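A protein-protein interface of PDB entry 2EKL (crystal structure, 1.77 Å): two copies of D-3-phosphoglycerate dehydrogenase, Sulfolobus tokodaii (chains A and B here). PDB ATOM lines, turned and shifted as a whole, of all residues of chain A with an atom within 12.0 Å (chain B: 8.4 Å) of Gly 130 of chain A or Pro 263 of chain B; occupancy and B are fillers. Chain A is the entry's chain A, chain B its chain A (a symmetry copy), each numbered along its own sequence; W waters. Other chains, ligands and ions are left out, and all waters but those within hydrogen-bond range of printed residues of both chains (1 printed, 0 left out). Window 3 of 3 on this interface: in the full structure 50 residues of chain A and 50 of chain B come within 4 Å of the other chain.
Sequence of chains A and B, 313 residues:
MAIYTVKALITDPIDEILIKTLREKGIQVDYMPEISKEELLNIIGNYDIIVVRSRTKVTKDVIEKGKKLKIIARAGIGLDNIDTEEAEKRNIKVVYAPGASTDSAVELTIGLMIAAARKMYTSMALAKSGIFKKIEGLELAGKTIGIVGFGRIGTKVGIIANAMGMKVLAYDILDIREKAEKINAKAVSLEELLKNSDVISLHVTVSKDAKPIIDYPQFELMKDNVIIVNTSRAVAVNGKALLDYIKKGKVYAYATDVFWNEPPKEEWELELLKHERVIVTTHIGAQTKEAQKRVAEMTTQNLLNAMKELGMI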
ATOM      1  N   TYR A 121     -24.175  32.275  -0.502  1.00  0.00           N
ATOM      2  CA  TYR A 121     -23.379  31.982  -1.688  1.00  0.00           C
ATOM      3  C   TYR A 121     -22.038  31.375  -1.302  1.00  0.00           C
ATOM      4  O   TYR A 121     -21.622  30.359  -1.853  1.00  0.00           O
ATOM      5  CB  TYR A 121     -23.134  33.246  -2.508  1.00  0.00           C
ATOM      6  CG  TYR A 121     -22.277  32.984  -3.725  1.00  0.00           C
ATOM      7  CD1 TYR A 121     -22.719  32.139  -4.741  1.00  0.00           C
ATOM      8  CD2 TYR A 121     -21.010  33.550  -3.842  1.00  0.00           C
ATOM      9  CE1 TYR A 121     -21.915  31.862  -5.850  1.00  0.00           C
ATOM     10  CE2 TYR A 121     -20.198  33.281  -4.945  1.00  0.00           C
ATOM     11  CZ  TYR A 121     -20.657  32.440  -5.940  1.00  0.00           C
ATOM     12  OH  TYR A 121     -19.860  32.187  -7.035  1.00  0.00           O
ATOM     13  N   THR A 122     -21.363  32.013  -0.357  1.00  0.00           N
ATOM     14  CA  THR A 122     -20.065  31.541   0.095  1.00  0.00           C
ATOM     15  C   THR A 122     -20.171  30.107   0.609  1.00  0.00           C
ATOM     16  O   THR A 122     -19.340  29.255   0.281  1.00  0.00           O
ATOM     17  CB  THR A 122     -19.514  32.449   1.208  1.00  0.00           C
ATOM     18  OG1 THR A 122     -19.408  33.793   0.717  1.00  0.00           O
ATOM     19  CG2 THR A 122     -18.140  31.966   1.661  1.00  0.00           C
ATOM     20  N   SER A 123     -21.207  29.847   1.399  1.00  0.00           N
ATOM     21  CA  SER A 123     -21.438  28.523   1.969  1.00  0.00           C
ATOM     22  C   SER A 123     -21.733  27.483   0.889  1.00  0.00           C
ATOM     23  O   SER A 123     -21.199  26.371   0.925  1.00  0.00           O
ATOM     24  CB  SER A 123     -22.606  28.585   2.961  1.00  0.00           C
ATOM     25  OG  SER A 123     -22.770  27.360   3.664  1.00  0.00           O
ATOM     26  N   MET A 124     -22.579  27.841  -0.076  1.00  0.00           N
ATOM     27  CA  MET A 124     -22.931  26.905  -1.136  1.00  0.00           C
ATOM     28  C   MET A 124     -21.732  26.584  -2.019  1.00  0.00           C
ATOM     29  O   MET A 124     -21.575  25.447  -2.476  1.00  0.00           O
ATOM     30  CB  MET A 124     -24.073  27.459  -1.989  1.00  0.00           C
ATOM     31  CG  MET A 124     -25.372  27.649  -1.227  1.00  0.00           C
ATOM     32  SD  MET A 124     -26.657  28.319  -2.302  1.00  0.00           S
ATOM     33  CE  MET A 124     -26.226  30.005  -2.322  1.00  0.00           C
ATOM     34  N   ALA A 125     -20.885  27.582  -2.255  1.00  0.00           N
ATOM     35  CA  ALA A 125     -19.696  27.370  -3.076  1.00  0.00           C
ATOM     36  C   ALA A 125     -18.768  26.407  -2.342  1.00  0.00           C
ATOM     37  O   ALA A 125     -18.203  25.487  -2.940  1.00  0.00           O
ATOM     38  CB  ALA A 125     -18.988  28.691  -3.331  1.00  0.00           C
ATOM     39  N   LEU A 126     -18.610  26.624  -1.041  1.00  0.00           N
ATOM     40  CA  LEU A 126     -17.769  25.759  -0.231  1.00  0.00           C
ATOM     41  C   LEU A 126     -18.289  24.327  -0.282  1.00  0.00           C
ATOM     42  O   LEU A 126     -17.533  23.396  -0.540  1.00  0.00           O
ATOM     43  CB  LEU A 126     -17.736  26.254   1.215  1.00  0.00           C
ATOM     44  CG  LEU A 126     -16.822  27.457   1.457  1.00  0.00           C
ATOM     45  CD1 LEU A 126     -17.143  28.115   2.783  1.00  0.00           C
ATOM     46  CD2 LEU A 126     -15.372  26.986   1.421  1.00  0.00           C
ATOM     47  N   ALA A 127     -19.588  24.158  -0.051  1.00  0.00           N
ATOM     48  CA  ALA A 127     -20.198  22.832  -0.073  1.00  0.00           C
ATOM     49  C   ALA A 127     -19.936  22.088  -1.384  1.00  0.00           C
ATOM     50  O   ALA A 127     -19.503  20.932  -1.376  1.00  0.00           O
ATOM     51  CB  ALA A 127     -21.708  22.945   0.174  1.00  0.00           C
ATOM     52  N   LYS A 128     -20.202  22.748  -2.507  1.00  0.00           N
ATOM     53  CA  LYS A 128     -19.999  22.124  -3.808  1.00  0.00           C
ATOM     54  C   LYS A 128     -18.546  21.694  -4.014  1.00  0.00           C
ATOM     55  O   LYS A 128     -18.272  20.758  -4.769  1.00  0.00           O
ATOM     56  CB  LYS A 128     -20.434  23.076  -4.924  1.00  0.00           C
ATOM     57  CG  LYS A 128     -21.951  23.251  -5.032  1.00  0.00           C
ATOM     58  CD  LYS A 128     -22.618  21.984  -5.553  1.00  0.00           C
ATOM     59  CE  LYS A 128     -24.120  22.189  -5.747  1.00  0.00           C
ATOM     60  NZ  LYS A 128     -24.769  21.025  -6.415  1.00  0.00           N
ATOM     61  N   SER A 129     -17.622  22.365  -3.336  1.00  0.00           N
ATOM     62  CA  SER A 129     -16.203  22.027  -3.453  1.00  0.00           C
ATOM     63  C   SER A 129     -15.819  20.921  -2.471  1.00  0.00           C
ATOM     64  O   SER A 129     -14.662  20.493  -2.420  1.00  0.00           O
ATOM     65  CB  SER A 129     -15.335  23.262  -3.196  1.00  0.00           C
ATOM     66  OG  SER A 129     -15.337  23.618  -1.825  1.00  0.00           O
ATOM     67  N   GLY A 130     -16.791  20.461  -1.689  1.00  0.00           N
ATOM     68  CA  GLY A 130     -16.525  19.404  -0.729  1.00  0.00           C
ATOM     69  C   GLY A 130     -15.927  19.893   0.576  1.00  0.00           C
ATOM     70  O   GLY A 130     -15.388  19.104   1.355  1.00  0.00           O
ATOM     71  N   ILE A 131     -16.023  21.197   0.818  1.00  0.00           N
ATOM     72  CA  ILE A 131     -15.495  21.793   2.039  1.00  0.00           C
ATOM     73  C   ILE A 131     -16.672  22.269   2.880  1.00  0.00           C
ATOM     74  O   ILE A 131     -17.237  23.332   2.625  1.00  0.00           O
ATOM     75  CB  ILE A 131     -14.583  22.999   1.720  1.00  0.00           C
ATOM     76  CG1 ILE A 131     -13.432  22.552   0.811  1.00  0.00           C
ATOM     77  CG2 ILE A 131     -14.049  23.608   3.006  1.00  0.00           C
ATOM     78  CD1 ILE A 131     -12.540  21.475   1.412  1.00  0.00           C
ATOM     79  N   PHE A 132     -17.045  21.480   3.882  1.00  0.00           N
ATOM     80  CA  PHE A 132     -18.172  21.841   4.728  1.00  0.00           C
ATOM     81  C   PHE A 132     -17.778  22.631   5.961  1.00  0.00           C
ATOM     82  O   PHE A 132     -17.891  22.161   7.095  1.00  0.00           O
ATOM     83  CB  PHE A 132     -18.962  20.589   5.102  1.00  0.00           C
ATOM     84  CG  PHE A 132     -19.871  20.113   4.004  1.00  0.00           C
ATOM     85  CD1 PHE A 132     -19.367  19.849   2.733  1.00  0.00           C
ATOM     86  CD2 PHE A 132     -21.233  19.958   4.230  1.00  0.00           C
ATOM     87  CE1 PHE A 132     -20.206  19.439   1.704  1.00  0.00           C
ATOM     88  CE2 PHE A 132     -22.081  19.546   3.207  1.00  0.00           C
ATOM     89  CZ  PHE A 132     -21.568  19.288   1.943  1.00  0.00           C
ATOM     90  N   LYS A 133     -17.308  23.847   5.713  1.00  0.00           N
ATOM     91  CA  LYS A 133     -16.897  24.763   6.764  1.00  0.00           C
ATOM     92  C   LYS A 133     -18.043  25.723   7.048  1.00  0.00           C
ATOM     93  O   LYS A 133     -18.594  26.327   6.129  1.00  0.00           O
ATOM     94  CB  LYS A 133     -15.669  25.549   6.314  1.00  0.00           C
ATOM     95  CG  LYS A 133     -15.232  26.632   7.283  1.00  0.00           C
ATOM     96  CD  LYS A 133     -13.892  27.220   6.874  1.00  0.00           C
ATOM     97  CE  LYS A 133     -13.943  27.842   5.492  1.00  0.00           C
ATOM     98  NZ  LYS A 133     -12.597  28.321   5.064  1.00  0.00           N
ATOM     99  N   LYS A 134     -18.401  25.860   8.319  1.00  0.00           N
ATOM    100  CA  LYS A 134     -19.485  26.753   8.713  1.00  0.00           C
ATOM    101  C   LYS A 134     -19.096  28.223   8.560  1.00  0.00           C
ATOM    102  O   LYS A 134     -17.935  28.590   8.730  1.00  0.00           O
ATOM    103  CB  LYS A 134     -19.890  26.482  10.162  1.00  0.00           C
ATOM    104  CG  LYS A 134     -20.463  25.091  10.406  1.00  0.00           C
ATOM    105  CD  LYS A 134     -20.863  24.918  11.866  1.00  0.00           C
ATOM    106  CE  LYS A 134     -21.487  23.554  12.121  1.00  0.00           C
ATOM    107  NZ  LYS A 134     -21.799  23.351  13.565  1.00  0.00           N
ATOM    108  N   PHE B 259     -26.371  17.271   5.616  1.00  0.00           N
ATOM    109  CA  PHE B 259     -26.018  16.154   4.749  1.00  0.00           C
ATOM    110  C   PHE B 259     -25.695  14.939   5.612  1.00  0.00           C
ATOM    111  O   PHE B 259     -25.222  15.075   6.739  1.00  0.00           O
ATOM    112  CB  PHE B 259     -24.811  16.515   3.876  1.00  0.00           C
ATOM    113  CG  PHE B 259     -25.044  16.308   2.403  1.00  0.00           C
ATOM    114  CD1 PHE B 259     -26.001  17.058   1.724  1.00  0.00           C
ATOM    115  CD2 PHE B 259     -24.309  15.360   1.693  1.00  0.00           C
ATOM    116  CE1 PHE B 259     -26.225  16.866   0.360  1.00  0.00           C
ATOM    117  CE2 PHE B 259     -24.524  15.163   0.331  1.00  0.00           C
ATOM    118  CZ  PHE B 259     -25.484  15.916  -0.337  1.00  0.00           C
ATOM    119  N   TRP B 260     -25.967  13.753   5.079  1.00  0.00           N
ATOM    120  CA  TRP B 260     -25.726  12.510   5.800  1.00  0.00           C
ATOM    121  C   TRP B 260     -24.303  12.486   6.340  1.00  0.00           C
ATOM    122  O   TRP B 260     -24.063  12.051   7.465  1.00  0.00           O
ATOM    123  CB  TRP B 260     -26.010  11.337   4.864  1.00  0.00           C
ATOM    124  CG  TRP B 260     -27.439  11.373   4.387  1.00  0.00           C
ATOM    125  CD1 TRP B 260     -28.520  10.784   4.983  1.00  0.00           C
ATOM    126  CD2 TRP B 260     -27.952  12.126   3.281  1.00  0.00           C
ATOM    127  NE1 TRP B 260     -29.676  11.129   4.320  1.00  0.00           N
ATOM    128  CE2 TRP B 260     -29.357  11.952   3.272  1.00  0.00           C
ATOM    129  CE3 TRP B 260     -27.366  12.935   2.299  1.00  0.00           C
ATOM    130  CZ2 TRP B 260     -30.181  12.559   2.319  1.00  0.00           C
ATOM    131  CZ3 TRP B 260     -28.188  13.539   1.350  1.00  0.00           C
ATOM    132  CH2 TRP B 260     -29.582  13.346   1.369  1.00  0.00           C
ATOM    133  N   ASN B 261     -23.372  12.979   5.530  1.00  0.00           N
ATOM    134  CA  ASN B 261     -21.965  13.084   5.901  1.00  0.00           C
ATOM    135  C   ASN B 261     -21.499  14.449   5.410  1.00  0.00           C
ATOM    136  O   ASN B 261     -21.661  14.779   4.235  1.00  0.00           O
ATOM    137  CB  ASN B 261     -21.137  11.979   5.241  1.00  0.00           C
ATOM    138  CG  ASN B 261     -21.225  10.660   5.986  1.00  0.00           C
ATOM    139  OD1 ASN B 261     -20.775  10.546   7.126  1.00  0.00           O
ATOM    140  ND2 ASN B 261     -21.813   9.656   5.345  1.00  0.00           N
ATOM    141  N   GLU B 262     -20.930  15.241   6.315  1.00  0.00           N
ATOM    142  CA  GLU B 262     -20.462  16.582   5.977  1.00  0.00           C
ATOM    143  C   GLU B 262     -18.958  16.714   6.224  1.00  0.00           C
ATOM    144  O   GLU B 262     -18.525  16.853   7.366  1.00  0.00           O
ATOM    145  CB  GLU B 262     -21.224  17.613   6.823  1.00  0.00           C
ATOM    146  CG  GLU B 262     -22.746  17.422   6.796  1.00  0.00           C
ATOM    147  CD  GLU B 262     -23.488  18.272   7.823  1.00  0.00           C
ATOM    148  OE1 GLU B 262     -22.843  18.834   8.729  1.00  0.00           O
ATOM    149  OE2 GLU B 262     -24.731  18.366   7.730  1.00  0.00           O
ATOM    150  N   PRO B 263     -18.139  16.668   5.156  1.00  0.00           N
ATOM    151  CA  PRO B 263     -18.477  16.505   3.737  1.00  0.00           C
ATOM    152  C   PRO B 263     -18.867  15.063   3.419  1.00  0.00           C
ATOM    153  O   PRO B 263     -18.614  14.157   4.213  1.00  0.00           O
ATOM    154  CB  PRO B 263     -17.183  16.896   3.014  1.00  0.00           C
ATOM    155  CG  PRO B 263     -16.371  17.626   4.059  1.00  0.00           C
ATOM    156  CD  PRO B 263     -16.691  16.876   5.309  1.00  0.00           C
ATOM    157  N   PRO B 264     -19.478  14.835   2.242  1.00  0.00           N
ATOM    158  CA  PRO B 264     -19.909  13.504   1.796  1.00  0.00           C
ATOM    159  C   PRO B 264     -18.725  12.569   1.574  1.00  0.00           C
ATOM    160  O   PRO B 264     -17.642  13.010   1.188  1.00  0.00           O
ATOM    161  CB  PRO B 264     -20.644  13.796   0.489  1.00  0.00           C
ATOM    162  CG  PRO B 264     -21.125  15.196   0.668  1.00  0.00           C
ATOM    163  CD  PRO B 264     -19.940  15.867   1.300  1.00  0.00           C
ATOM    164  N   LYS B 265     -18.940  11.278   1.806  1.00  0.00           N
ATOM    165  CA  LYS B 265     -17.885  10.289   1.629  1.00  0.00           C
ATOM    166  C   LYS B 265     -18.312   9.144   0.714  1.00  0.00           C
ATOM    167  O   LYS B 265     -17.506   8.626  -0.060  1.00  0.00           O
ATOM    168  CB  LYS B 265     -17.457   9.735   2.990  1.00  0.00           C
ATOM    169  CG  LYS B 265     -16.873  10.785   3.924  1.00  0.00           C
ATOM    170  CD  LYS B 265     -16.430  10.187   5.253  1.00  0.00           C
ATOM    171  CE  LYS B 265     -17.606   9.644   6.048  1.00  0.00           C
ATOM    172  NZ  LYS B 265     -17.167   9.099   7.363  1.00  0.00           N
ATOM    173  N   GLU B 266     -19.583   8.762   0.796  1.00  0.00           N
ATOM    174  CA  GLU B 266     -20.116   7.670  -0.014  1.00  0.00           C
ATOM    175  C   GLU B 266     -20.384   8.099  -1.457  1.00  0.00           C
ATOM    176  O   GLU B 266     -20.704   9.260  -1.720  1.00  0.00           O
ATOM    177  CB  GLU B 266     -21.403   7.136   0.623  1.00  0.00           C
ATOM    178  CG  GLU B 266     -21.243   6.764   2.093  1.00  0.00           C
ATOM    179  CD  GLU B 266     -22.457   6.046   2.656  1.00  0.00           C
ATOM    180  OE1 GLU B 266     -22.848   5.009   2.083  1.00  0.00           O
ATOM    181  OE2 GLU B 266     -23.017   6.513   3.675  1.00  0.00           O
ATOM    182  N   GLU B 269     -23.692   9.784  -2.138  1.00  0.00           N
ATOM    183  CA  GLU B 269     -23.727  11.097  -1.491  1.00  0.00           C
ATOM    184  C   GLU B 269     -23.011  12.110  -2.366  1.00  0.00           C
ATOM    185  O   GLU B 269     -23.449  13.248  -2.520  1.00  0.00           O
ATOM    186  CB  GLU B 269     -23.021  11.058  -0.138  1.00  0.00           C
ATOM    187  CG  GLU B 269     -23.868  10.614   1.021  1.00  0.00           C
ATOM    188  CD  GLU B 269     -23.200  10.921   2.341  1.00  0.00           C
ATOM    189  OE1 GLU B 269     -22.181  10.273   2.654  1.00  0.00           O
ATOM    190  OE2 GLU B 269     -23.683  11.826   3.052  1.00  0.00           O
ATOM    191  N   LEU B 270     -21.877  11.691  -2.913  1.00  0.00           N
ATOM    192  CA  LEU B 270     -21.097  12.547  -3.785  1.00  0.00           C
ATOM    193  C   LEU B 270     -21.889  12.879  -5.047  1.00  0.00           C
ATOM    194  O   LEU B 270     -21.841  14.005  -5.536  1.00  0.00           O
ATOM    195  CB  LEU B 270     -19.786  11.846  -4.151  1.00  0.00           C
ATOM    196  CG  LEU B 270     -18.869  11.623  -2.946  1.00  0.00           C
ATOM    197  CD1 LEU B 270     -17.707  10.710  -3.320  1.00  0.00           C
ATOM    198  CD2 LEU B 270     -18.369  12.974  -2.454  1.00  0.00           C
ATOM    199  N   LEU B 273     -24.453  15.566  -4.101  1.00  0.00           N
ATOM    200  CA  LEU B 273     -23.805  16.857  -3.909  1.00  0.00           C
ATOM    201  C   LEU B 273     -23.481  17.585  -5.212  1.00  0.00           C
ATOM    202  O   LEU B 273     -23.690  18.793  -5.316  1.00  0.00           O
ATOM    203  CB  LEU B 273     -22.524  16.693  -3.084  1.00  0.00           C
ATOM    204  CG  LEU B 273     -21.728  17.978  -2.827  1.00  0.00           C
ATOM    205  CD1 LEU B 273     -22.585  18.963  -2.040  1.00  0.00           C
ATOM    206  CD2 LEU B 273     -20.455  17.656  -2.069  1.00  0.00           C
ATOM    207  N   THR B 282     -23.544  24.651   4.340  1.00  0.00           N
ATOM    208  CA  THR B 282     -22.711  23.892   5.263  1.00  0.00           C
ATOM    209  C   THR B 282     -23.124  23.831   6.735  1.00  0.00           C
ATOM    210  O   THR B 282     -22.309  24.064   7.631  1.00  0.00           O
ATOM    211  CB  THR B 282     -21.260  24.400   5.144  1.00  0.00           C
ATOM    212  OG1 THR B 282     -21.223  25.805   5.409  1.00  0.00           O
ATOM    213  CG2 THR B 282     -20.742  24.175   3.727  1.00  0.00           C
HETATM  214  O   HOH W   1     -20.720  21.661   8.170  1.00  0.00           O
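OG of Ser 123 of chain A sits at hydrogen-bond distance from OG1 of Thr 282 of chain B, at 2.8 Å. The side-chain amino group of Lys 128 of chain A lies within hydrogen-bond range of the backbone carbonyl oxygen of Leu 273 of chain B, 2.7 Å away. The backbone carbonyl oxygen of Lys 133 of chain A sits at hydrogen-bond distance from the side-chain hydroxyl of Thr 282 of chain B, 2.8 Å away.
The backbone carbonyl oxygen of Leu 126 of chain A is in hydrogen-bond range of the backbone NH of Ile 131 of chain A (3.0 Å). The backbone NH (N) of Phe 259 of chain B is in hydrogen-bond range of the side-chain carboxylate (OE2) of Glu 262 of chain B, at 2.9 Å.
Among the printed residues, pairs that only touch across the chains: Ala 127 of chain A with Leu 273 of chain B, Ala 127 of chain A with Thr 282 of chain B, Gly 130 of chain A with Pro 263 of chain B, Ile 131 of chain A with Thr 282 of chain B, Phe 132 of chain A with Glu 262 of chain B, Phe 132 of chain A with Pro 263 of chain B, Phe 132 of chain A with Pro 264 of chain B, Phe 132 of chain A with Thr 282 of chain B and Lys 134 of chain A with Thr 282 of chain B.
Tyr 121 of chain A touches none of the printed residues of chain B. Of the printed residues of chain B, Ser 123 of chain A touches Thr 282 (2.8 Å). Of the printed residues of chain B, Ala 127 of chain A touches Leu 273 (3.5 Å) and Thr 282 (3.9 Å). No residue of chain B comes within 4 Å of Ser 129 of chain A. Glu 262 of chain B touches one residue of chain A. Printed residues of chain A within 4 Å of Pro 263 of chain B: Gly 130 and Phe 132. Pro 264 of chain B touches just one residue of chain A: Phe 132 (3.6 Å). No residue of chain A comes within 4 Å of Lys 265 of chain B. Printed residues of chain A within 4 Å of Leu 273 of chain B: Ala 127 and Lys 128. The nearest residue of chain B that does not touch Gly 130 of chain A is Leu 273 of chain B (4.5 Å). The nearest printed residue of chain B that does not touch Lys 134 of chain A is Glu 262 of chain B (6.0 Å).
Of the 12 printed residues of chain B, 5 touch a printed residue of chain A. Hydrophobic or aromatic side chains of chain B within 4 Å of the printed part of chain A: Pro 263, Pro 264 and Leu 273. Printed residues of chain A that touch a printed residue of chain B: Ser 123, Ala 127, Lys 128, Gly 130, Ile 131, Phe 132, Lys 133 and Lys 134.
No position is printed for both chains.
Water W1 bridges O of Thr 282 of chain B (2.9 Å) and O of Phe 132 of chain A (3.1 Å).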
